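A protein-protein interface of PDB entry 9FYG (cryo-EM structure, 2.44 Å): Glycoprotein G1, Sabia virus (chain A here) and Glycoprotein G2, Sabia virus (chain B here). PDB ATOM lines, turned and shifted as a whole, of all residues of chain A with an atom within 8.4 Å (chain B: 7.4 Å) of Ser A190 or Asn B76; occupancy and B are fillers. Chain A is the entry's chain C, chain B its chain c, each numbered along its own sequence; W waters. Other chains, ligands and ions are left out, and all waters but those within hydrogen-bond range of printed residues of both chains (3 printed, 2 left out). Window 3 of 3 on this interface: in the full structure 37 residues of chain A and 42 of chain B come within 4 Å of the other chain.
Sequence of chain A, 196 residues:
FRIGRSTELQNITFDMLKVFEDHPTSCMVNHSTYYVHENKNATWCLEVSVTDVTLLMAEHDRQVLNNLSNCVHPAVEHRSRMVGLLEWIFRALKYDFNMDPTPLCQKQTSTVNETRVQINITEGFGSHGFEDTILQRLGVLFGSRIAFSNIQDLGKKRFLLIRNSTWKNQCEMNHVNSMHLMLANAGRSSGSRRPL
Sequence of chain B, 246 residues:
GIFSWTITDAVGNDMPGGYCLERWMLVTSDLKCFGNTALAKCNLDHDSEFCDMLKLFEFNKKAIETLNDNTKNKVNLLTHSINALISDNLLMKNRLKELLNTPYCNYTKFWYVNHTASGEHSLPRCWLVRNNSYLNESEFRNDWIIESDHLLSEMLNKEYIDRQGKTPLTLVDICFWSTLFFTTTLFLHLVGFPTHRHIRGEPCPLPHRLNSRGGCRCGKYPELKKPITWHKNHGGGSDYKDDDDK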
ATOM      1  N   LYS A  18      -7.227  23.945   2.853  1.00  0.00           N
ATOM      2  CA  LYS A  18      -6.626  22.892   3.668  1.00  0.00           C
ATOM      3  C   LYS A  18      -5.107  22.891   3.569  1.00  0.00           C
ATOM      4  O   LYS A  18      -4.425  22.420   4.487  1.00  0.00           O
ATOM      5  CB  LYS A  18      -7.177  21.527   3.254  1.00  0.00           C
ATOM      6  CG  LYS A  18      -8.505  21.164   3.890  1.00  0.00           C
ATOM      7  CD  LYS A  18      -9.163  20.013   3.147  1.00  0.00           C
ATOM      8  CE  LYS A  18      -8.471  18.693   3.455  1.00  0.00           C
ATOM      9  NZ  LYS A  18      -9.428  17.552   3.496  1.00  0.00           N
ATOM     10  N   VAL A  19      -4.560  23.405   2.469  1.00  0.00           N
ATOM     11  CA  VAL A  19      -3.111  23.498   2.335  1.00  0.00           C
ATOM     12  C   VAL A  19      -2.550  24.554   3.281  1.00  0.00           C
ATOM     13  O   VAL A  19      -1.469  24.380   3.853  1.00  0.00           O
ATOM     14  CB  VAL A  19      -2.731  23.780   0.868  1.00  0.00           C
ATOM     15  CG1 VAL A  19      -1.219  23.826   0.704  1.00  0.00           C
ATOM     16  CG2 VAL A  19      -3.339  22.728  -0.044  1.00  0.00           C
ATOM     17  N   PHE A  20      -3.273  25.660   3.471  1.00  0.00           N
ATOM     18  CA  PHE A  20      -2.746  26.808   4.202  1.00  0.00           C
ATOM     19  C   PHE A  20      -3.541  27.135   5.464  1.00  0.00           C
ATOM     20  O   PHE A  20      -3.427  28.249   5.983  1.00  0.00           O
ATOM     21  CB  PHE A  20      -2.685  28.031   3.284  1.00  0.00           C
ATOM     22  CG  PHE A  20      -1.652  27.926   2.202  1.00  0.00           C
ATOM     23  CD1 PHE A  20      -0.307  27.830   2.515  1.00  0.00           C
ATOM     24  CD2 PHE A  20      -2.023  27.926   0.869  1.00  0.00           C
ATOM     25  CE1 PHE A  20       0.646  27.736   1.519  1.00  0.00           C
ATOM     26  CE2 PHE A  20      -1.073  27.832  -0.129  1.00  0.00           C
ATOM     27  CZ  PHE A  20       0.261  27.736   0.196  1.00  0.00           C
ATOM     28  N   GLU A  21      -4.342  26.197   5.974  1.00  0.00           N
ATOM     29  CA  GLU A  21      -5.079  26.452   7.212  1.00  0.00           C
ATOM     30  C   GLU A  21      -4.141  26.677   8.391  1.00  0.00           C
ATOM     31  O   GLU A  21      -4.354  27.590   9.197  1.00  0.00           O
ATOM     32  CB  GLU A  21      -6.029  25.294   7.522  1.00  0.00           C
ATOM     33  CG  GLU A  21      -7.233  25.176   6.618  1.00  0.00           C
ATOM     34  CD  GLU A  21      -8.103  23.987   6.969  1.00  0.00           C
ATOM     35  OE1 GLU A  21      -7.677  23.170   7.810  1.00  0.00           O
ATOM     36  OE2 GLU A  21      -9.216  23.875   6.414  1.00  0.00           O
ATOM     37  N   ASP A  22      -3.100  25.859   8.512  1.00  0.00           N
ATOM     38  CA  ASP A  22      -2.278  25.825   9.712  1.00  0.00           C
ATOM     39  C   ASP A  22      -1.015  26.667   9.608  1.00  0.00           C
ATOM     40  O   ASP A  22      -0.203  26.656  10.538  1.00  0.00           O
ATOM     41  CB  ASP A  22      -1.909  24.377  10.047  1.00  0.00           C
ATOM     42  CG  ASP A  22      -3.106  23.447   9.987  1.00  0.00           C
ATOM     43  OD1 ASP A  22      -4.105  23.718  10.684  1.00  0.00           O
ATOM     44  OD2 ASP A  22      -3.049  22.448   9.241  1.00  0.00           O
ATOM     45  N   HIS A  23      -0.832  27.399   8.523  1.00  0.00           N
ATOM     46  CA  HIS A  23       0.377  28.171   8.304  1.00  0.00           C
ATOM     47  C   HIS A  23       0.087  29.665   8.369  1.00  0.00           C
ATOM     48  O   HIS A  23      -1.057  30.094   8.193  1.00  0.00           O
ATOM     49  CB  HIS A  23       0.996  27.815   6.947  1.00  0.00           C
ATOM     50  CG  HIS A  23       1.245  26.350   6.770  1.00  0.00           C
ATOM     51  ND1 HIS A  23       2.261  25.685   7.420  1.00  0.00           N
ATOM     52  CD2 HIS A  23       0.604  25.421   6.023  1.00  0.00           C
ATOM     53  CE1 HIS A  23       2.238  24.409   7.079  1.00  0.00           C
ATOM     54  NE2 HIS A  23       1.242  24.223   6.233  1.00  0.00           N
ATOM     55  N   PRO A  24       1.099  30.486   8.655  1.00  0.00           N
ATOM     56  CA  PRO A  24       0.886  31.937   8.657  1.00  0.00           C
ATOM     57  C   PRO A  24       0.404  32.431   7.302  1.00  0.00           C
ATOM     58  O   PRO A  24       0.858  31.973   6.252  1.00  0.00           O
ATOM     59  CB  PRO A  24       2.270  32.502   8.998  1.00  0.00           C
ATOM     60  CG  PRO A  24       2.979  31.398   9.678  1.00  0.00           C
ATOM     61  CD  PRO A  24       2.455  30.124   9.104  1.00  0.00           C
ATOM     62  N   GLU A  38      -1.298  34.208  12.377  1.00  0.00           N
ATOM     63  CA  GLU A  38      -0.418  33.084  12.681  1.00  0.00           C
ATOM     64  C   GLU A  38      -1.020  31.768  12.197  1.00  0.00           C
ATOM     65  O   GLU A  38      -0.302  30.904  11.681  1.00  0.00           O
ATOM     66  CB  GLU A  38      -0.116  33.073  14.181  1.00  0.00           C
ATOM     67  CG  GLU A  38       1.001  32.144  14.638  1.00  0.00           C
ATOM     68  CD  GLU A  38       0.511  30.767  15.020  1.00  0.00           C
ATOM     69  OE1 GLU A  38      -0.643  30.659  15.480  1.00  0.00           O
ATOM     70  OE2 GLU A  38       1.282  29.797  14.874  1.00  0.00           O
ATOM     71  N   ASN A  39      -2.330  31.606  12.341  1.00  0.00           N
ATOM     72  CA  ASN A  39      -3.069  30.539  11.676  1.00  0.00           C
ATOM     73  C   ASN A  39      -4.543  30.926  11.675  1.00  0.00           C
ATOM     74  O   ASN A  39      -4.919  32.003  12.141  1.00  0.00           O
ATOM     75  CB  ASN A  39      -2.830  29.175  12.333  1.00  0.00           C
ATOM     76  CG  ASN A  39      -3.204  29.155  13.797  1.00  0.00           C
ATOM     77  OD1 ASN A  39      -4.382  29.153  14.149  1.00  0.00           O
ATOM     78  ND2 ASN A  39      -2.200  29.122  14.660  1.00  0.00           N
ATOM     79  N   ARG A  81       4.366  32.530  20.342  1.00  0.00           N
ATOM     80  CA  ARG A  81       3.846  32.560  18.980  1.00  0.00           C
ATOM     81  C   ARG A  81       3.911  33.963  18.388  1.00  0.00           C
ATOM     82  O   ARG A  81       4.181  34.124  17.193  1.00  0.00           O
ATOM     83  CB  ARG A  81       2.415  32.026  18.956  1.00  0.00           C
ATOM     84  CG  ARG A  81       2.307  30.539  19.246  1.00  0.00           C
ATOM     85  CD  ARG A  81       0.865  30.076  19.226  1.00  0.00           C
ATOM     86  NE  ARG A  81       0.742  28.645  19.470  1.00  0.00           N
ATOM     87  CZ  ARG A  81       0.821  27.714  18.528  1.00  0.00           C
ATOM     88  NH1 ARG A  81       1.034  28.028  17.263  1.00  0.00           N
ATOM     89  NH2 ARG A  81       0.685  26.436  18.868  1.00  0.00           N
ATOM     90  N   TRP A  88       8.931  35.858  11.624  1.00  0.00           N
ATOM     91  CA  TRP A  88       8.468  35.516  10.280  1.00  0.00           C
ATOM     92  C   TRP A  88       8.289  36.773   9.433  1.00  0.00           C
ATOM     93  O   TRP A  88       8.650  36.791   8.251  1.00  0.00           O
ATOM     94  CB  TRP A  88       7.163  34.713  10.377  1.00  0.00           C
ATOM     95  CG  TRP A  88       7.328  33.292  10.893  1.00  0.00           C
ATOM     96  CD1 TRP A  88       7.427  32.913  12.189  1.00  0.00           C
ATOM     97  CD2 TRP A  88       7.231  32.076  10.140  1.00  0.00           C
ATOM     98  NE1 TRP A  88       7.510  31.556  12.295  1.00  0.00           N
ATOM     99  CE2 TRP A  88       7.376  31.011  11.049  1.00  0.00           C
ATOM    100  CE3 TRP A  88       7.058  31.782   8.790  1.00  0.00           C
ATOM    101  CZ2 TRP A  88       7.364  29.682  10.652  1.00  0.00           C
ATOM    102  CZ3 TRP A  88       7.056  30.459   8.401  1.00  0.00           C
ATOM    103  CH2 TRP A  88       7.207  29.427   9.323  1.00  0.00           C
ATOM    104  N   MET A 182       5.729  32.086   3.166  1.00  0.00           N
ATOM    105  CA  MET A 182       6.408  30.819   3.413  1.00  0.00           C
ATOM    106  C   MET A 182       7.716  30.715   2.642  1.00  0.00           C
ATOM    107  O   MET A 182       8.691  30.162   3.160  1.00  0.00           O
ATOM    108  CB  MET A 182       5.491  29.655   3.046  1.00  0.00           C
ATOM    109  CG  MET A 182       4.430  29.355   4.084  1.00  0.00           C
ATOM    110  SD  MET A 182       3.450  27.896   3.697  1.00  0.00           S
ATOM    111  CE  MET A 182       4.195  26.694   4.791  1.00  0.00           C
ATOM    112  N   ASN A 185      10.429  32.246   4.382  1.00  0.00           N
ATOM    113  CA  ASN A 185      10.685  31.608   5.670  1.00  0.00           C
ATOM    114  C   ASN A 185      10.912  30.108   5.515  1.00  0.00           C
ATOM    115  O   ASN A 185      10.445  29.302   6.325  1.00  0.00           O
ATOM    116  CB  ASN A 185       9.537  31.866   6.640  1.00  0.00           C
ATOM    117  CG  ASN A 185       9.543  33.270   7.204  1.00  0.00           C
ATOM    118  OD1 ASN A 185      10.283  33.569   8.134  1.00  0.00           O
ATOM    119  ND2 ASN A 185       8.709  34.136   6.647  1.00  0.00           N
ATOM    120  N   GLY A 187      12.241  26.508   5.785  1.00  0.00           N
ATOM    121  CA  GLY A 187      12.923  25.779   6.827  1.00  0.00           C
ATOM    122  C   GLY A 187      12.430  26.058   8.230  1.00  0.00           C
ATOM    123  O   GLY A 187      12.721  25.277   9.140  1.00  0.00           O
ATOM    124  N   ARG A 188      11.682  27.136   8.434  1.00  0.00           N
ATOM    125  CA  ARG A 188      11.152  27.449   9.753  1.00  0.00           C
ATOM    126  C   ARG A 188       9.878  26.648   9.994  1.00  0.00           C
ATOM    127  O   ARG A 188       8.953  26.674   9.178  1.00  0.00           O
ATOM    128  CB  ARG A 188      10.878  28.948   9.882  1.00  0.00           C
ATOM    129  CG  ARG A 188      12.127  29.808   9.898  1.00  0.00           C
ATOM    130  CD  ARG A 188      12.945  29.556  11.150  1.00  0.00           C
ATOM    131  NE  ARG A 188      14.328  29.991  11.004  1.00  0.00           N
ATOM    132  CZ  ARG A 188      15.170  30.172  12.013  1.00  0.00           C
ATOM    133  NH1 ARG A 188      14.804  29.964  13.266  1.00  0.00           N
ATOM    134  NH2 ARG A 188      16.412  30.572  11.756  1.00  0.00           N
ATOM    135  N   SER A 189       9.830  25.944  11.121  1.00  0.00           N
ATOM    136  CA  SER A 189       8.717  25.044  11.396  1.00  0.00           C
ATOM    137  C   SER A 189       7.398  25.801  11.515  1.00  0.00           C
ATOM    138  O   SER A 189       7.333  26.891  12.090  1.00  0.00           O
ATOM    139  CB  SER A 189       8.989  24.252  12.676  1.00  0.00           C
ATOM    140  OG  SER A 189       8.556  24.959  13.823  1.00  0.00           O
ATOM    141  N   SER A 190       6.343  25.205  10.962  1.00  0.00           N
ATOM    142  CA  SER A 190       4.992  25.741  11.055  1.00  0.00           C
ATOM    143  C   SER A 190       4.007  24.599  10.844  1.00  0.00           C
ATOM    144  O   SER A 190       4.373  23.512  10.392  1.00  0.00           O
ATOM    145  CB  SER A 190       4.756  26.864  10.040  1.00  0.00           C
ATOM    146  OG  SER A 190       4.854  26.386   8.710  1.00  0.00           O
ATOM    147  N   GLY A 191       2.747  24.861  11.180  1.00  0.00           N
ATOM    148  CA  GLY A 191       1.694  23.887  10.968  1.00  0.00           C
ATOM    149  C   GLY A 191       1.417  23.016  12.174  1.00  0.00           C
ATOM    150  O   GLY A 191       2.273  22.231  12.593  1.00  0.00           O
ATOM    151  N   SER A 192       0.221  23.141  12.741  1.00  0.00           N
ATOM    152  CA  SER A 192      -0.164  22.345  13.902  1.00  0.00           C
ATOM    153  C   SER A 192      -1.502  21.656  13.666  1.00  0.00           C
ATOM    154  O   SER A 192      -2.535  22.315  13.538  1.00  0.00           O
ATOM    155  CB  SER A 192      -0.237  23.220  15.154  1.00  0.00           C
ATOM    156  OG  SER A 192       1.047  23.686  15.530  1.00  0.00           O
ATOM    157  N   PHE B  59       1.776  17.026  -2.491  1.00  0.00           N
ATOM    158  CA  PHE B  59       2.536  16.993  -1.245  1.00  0.00           C
ATOM    159  C   PHE B  59       1.607  17.067  -0.037  1.00  0.00           C
ATOM    160  O   PHE B  59       1.755  16.301   0.924  1.00  0.00           O
ATOM    161  CB  PHE B  59       3.549  18.137  -1.221  1.00  0.00           C
ATOM    162  CG  PHE B  59       4.493  18.093  -0.052  1.00  0.00           C
ATOM    163  CD1 PHE B  59       5.696  17.415  -0.142  1.00  0.00           C
ATOM    164  CD2 PHE B  59       4.179  18.733   1.135  1.00  0.00           C
ATOM    165  CE1 PHE B  59       6.563  17.372   0.929  1.00  0.00           C
ATOM    166  CE2 PHE B  59       5.044  18.693   2.209  1.00  0.00           C
ATOM    167  CZ  PHE B  59       6.236  18.011   2.107  1.00  0.00           C
ATOM    168  N   ASN B  60       0.629  17.974  -0.077  1.00  0.00           N
ATOM    169  CA  ASN B  60      -0.297  18.105   1.044  1.00  0.00           C
ATOM    170  C   ASN B  60      -1.145  16.850   1.216  1.00  0.00           C
ATOM    171  O   ASN B  60      -1.414  16.427   2.346  1.00  0.00           O
ATOM    172  CB  ASN B  60      -1.185  19.332   0.854  1.00  0.00           C
ATOM    173  CG  ASN B  60      -1.896  19.735   2.129  1.00  0.00           C
ATOM    174  OD1 ASN B  60      -3.051  19.374   2.350  1.00  0.00           O
ATOM    175  ND2 ASN B  60      -1.205  20.485   2.979  1.00  0.00           N
ATOM    176  N   ALA B  63       0.881  14.179   2.734  1.00  0.00           N
ATOM    177  CA  ALA B  63       1.127  14.501   4.135  1.00  0.00           C
ATOM    178  C   ALA B  63      -0.095  14.221   5.001  1.00  0.00           C
ATOM    179  O   ALA B  63       0.043  13.811   6.160  1.00  0.00           O
ATOM    180  CB  ALA B  63       1.549  15.964   4.271  1.00  0.00           C
ATOM    181  N   LYS B  74       2.600  14.647  14.911  1.00  0.00           N
ATOM    182  CA  LYS B  74       2.585  14.925  13.479  1.00  0.00           C
ATOM    183  C   LYS B  74       3.365  16.198  13.164  1.00  0.00           C
ATOM    184  O   LYS B  74       3.131  17.246  13.765  1.00  0.00           O
ATOM    185  CB  LYS B  74       1.148  15.045  12.972  1.00  0.00           C
ATOM    186  CG  LYS B  74       1.036  15.185  11.464  1.00  0.00           C
ATOM    187  CD  LYS B  74       1.603  13.968  10.754  1.00  0.00           C
ATOM    188  CE  LYS B  74       1.504  14.119   9.246  1.00  0.00           C
ATOM    189  NZ  LYS B  74       2.111  12.964   8.530  1.00  0.00           N
ATOM    190  N   VAL B  75       4.289  16.097  12.212  1.00  0.00           N
ATOM    191  CA  VAL B  75       5.169  17.197  11.833  1.00  0.00           C
ATOM    192  C   VAL B  75       4.830  17.620  10.411  1.00  0.00           C
ATOM    193  O   VAL B  75       4.768  16.781   9.505  1.00  0.00           O
ATOM    194  CB  VAL B  75       6.650  16.796  11.949  1.00  0.00           C
ATOM    195  CG1 VAL B  75       7.542  17.844  11.298  1.00  0.00           C
ATOM    196  CG2 VAL B  75       7.032  16.593  13.404  1.00  0.00           C
ATOM    197  N   ASN B  76       4.604  18.917  10.220  1.00  0.00           N
ATOM    198  CA  ASN B  76       4.372  19.480   8.898  1.00  0.00           C
ATOM    199  C   ASN B  76       5.706  19.863   8.275  1.00  0.00           C
ATOM    200  O   ASN B  76       6.496  20.593   8.882  1.00  0.00           O
ATOM    201  CB  ASN B  76       3.452  20.699   8.984  1.00  0.00           C
ATOM    202  CG  ASN B  76       2.484  20.786   7.823  1.00  0.00           C
ATOM    203  OD1 ASN B  76       2.881  20.725   6.661  1.00  0.00           O
ATOM    204  ND2 ASN B  76       1.202  20.933   8.133  1.00  0.00           N
ATOM    205  N   LEU B  77       5.958  19.364   7.066  1.00  0.00           N
ATOM    206  CA  LEU B  77       7.217  19.601   6.371  1.00  0.00           C
ATOM    207  C   LEU B  77       7.052  20.527   5.172  1.00  0.00           C
ATOM    208  O   LEU B  77       7.905  20.536   4.280  1.00  0.00           O
ATOM    209  CB  LEU B  77       7.833  18.272   5.930  1.00  0.00           C
ATOM    210  CG  LEU B  77       8.275  17.318   7.040  1.00  0.00           C
ATOM    211  CD1 LEU B  77       8.857  16.045   6.453  1.00  0.00           C
ATOM    212  CD2 LEU B  77       9.278  17.990   7.959  1.00  0.00           C
ATOM    213  N   LEU B  78       5.969  21.308   5.136  1.00  0.00           N
ATOM    214  CA  LEU B  78       5.695  22.145   3.972  1.00  0.00           C
ATOM    215  C   LEU B  78       6.748  23.232   3.786  1.00  0.00           C
ATOM    216  O   LEU B  78       7.064  23.593   2.648  1.00  0.00           O
ATOM    217  CB  LEU B  78       4.302  22.764   4.088  1.00  0.00           C
ATOM    218  CG  LEU B  78       3.795  23.523   2.860  1.00  0.00           C
ATOM    219  CD1 LEU B  78       4.045  22.725   1.591  1.00  0.00           C
ATOM    220  CD2 LEU B  78       2.326  23.864   3.002  1.00  0.00           C
ATOM    221  N   THR B  79       7.297  23.768   4.878  1.00  0.00           N
ATOM    222  CA  THR B  79       8.318  24.801   4.757  1.00  0.00           C
ATOM    223  C   THR B  79       9.641  24.258   4.231  1.00  0.00           C
ATOM    224  O   THR B  79      10.430  25.024   3.670  1.00  0.00           O
ATOM    225  CB  THR B  79       8.544  25.491   6.102  1.00  0.00           C
ATOM    226  OG1 THR B  79       8.961  24.528   7.077  1.00  0.00           O
ATOM    227  CG2 THR B  79       7.272  26.167   6.567  1.00  0.00           C
ATOM    228  N   HIS B  80       9.900  22.962   4.403  1.00  0.00           N
ATOM    229  CA  HIS B  80      11.122  22.368   3.876  1.00  0.00           C
ATOM    230  C   HIS B  80      11.045  22.131   2.374  1.00  0.00           C
ATOM    231  O   HIS B  80      12.079  22.135   1.699  1.00  0.00           O
ATOM    232  CB  HIS B  80      11.419  21.052   4.594  1.00  0.00           C
ATOM    233  CG  HIS B  80      11.753  21.221   6.043  1.00  0.00           C
ATOM    234  ND1 HIS B  80      12.895  21.859   6.472  1.00  0.00           N
ATOM    235  CD2 HIS B  80      11.088  20.846   7.159  1.00  0.00           C
ATOM    236  CE1 HIS B  80      12.922  21.864   7.793  1.00  0.00           C
ATOM    237  NE2 HIS B  80      11.837  21.255   8.234  1.00  0.00           N
HETATM  238  O   HOH W   1       0.020  22.068   4.580  1.00  0.00           O
HETATM  239  O   HOH W   2      -0.714  20.488  10.116  1.00  0.00           O
HETATM  240  O   HOH W   3       5.497  23.412   7.589  1.00  0.00           O
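The side-chain amide oxygen of Asn B76 lies close to the backbone NH of Leu B78 (3.5 Å). ND1 of His A23 lies within hydrogen-bond range of OG of Ser A190 (3.0 Å).
O of Thr B79 sits at hydrogen-bond distance from N of Gly A187, at 3.2 Å. OG1 of Thr B79 sits at hydrogen-bond distance from O of Arg A188, at 3.0 Å.
Of the printed residues of chain B, Lys A18 touches Asn B60 (3.97 Å). Phe A20 touches none of the printed residues of chain B. Printed residues of chain B within 4 Å of Arg A188: Thr B79. Printed residues of chain B within 4 Å of Ser A190: Asn B76 and Thr B79. No residue of chain B comes within 4 Å of Gly A191. Phe B59 touches none of the printed residues of chain A. Printed residues of chain A within 4 Å of Asn B60: Lys A18 (3.97 Å) and Val A19 (3.6 Å). Printed residues of chain A within 4 Å of Leu B78: Val A19, His A23 and Met A182. The nearest residue of chain B that does not touch Ser A190 is Leu B77 (5.5 Å).
Among the printed residues, pairs that only touch across the chains: Lys A18 with Asn B60 (3.97 Å), Val A19 with Asn B60 (3.6 Å), Val A19 with Leu B78 (3.9 Å), His A23 with Asn B76 (3.7 Å), His A23 with Leu B78 (3.4 Å), Met A182 with Leu B78 (3.7 Å), Met A182 with Thr B79 (3.6 Å), Gly A187 with His B80 (3.7 Å), Ser A190 with Asn B76 (3.3 Å) and Ser A190 with Thr B79 (3.2 Å).
Of the 19 printed residues of chain A, 7 touch a printed residue of chain B. Hydrophobic or aromatic side chains of chain A within 4 Å of the printed part of chain B: Val A19, His A23 and Met A182. Of the 10 printed residues of chain B, 5 touch a printed residue of chain A. Among the printed residues, 12 pairs touch across the chains.
Water W1 lies within hydrogen-bond range of the side-chain amide nitrogen (ND2) of Asn B60, the backbone carbonyl oxygen (O) of Val A19 and a ring nitrogen (NE2) of His A23. Water W2 lies within hydrogen-bond range of the side-chain amide nitrogen (ND2) of Asn B76 (2.8 Å) and the side-chain carboxylate (OD2) of Asp A22 (3.2 Å). Water W3 lies within hydrogen-bond range of the backbone carbonyl oxygen of Ser A190, the backbone carbonyl oxygen of Asn B76, the backbone NH of Leu B78 and the backbone NH of Thr B79.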
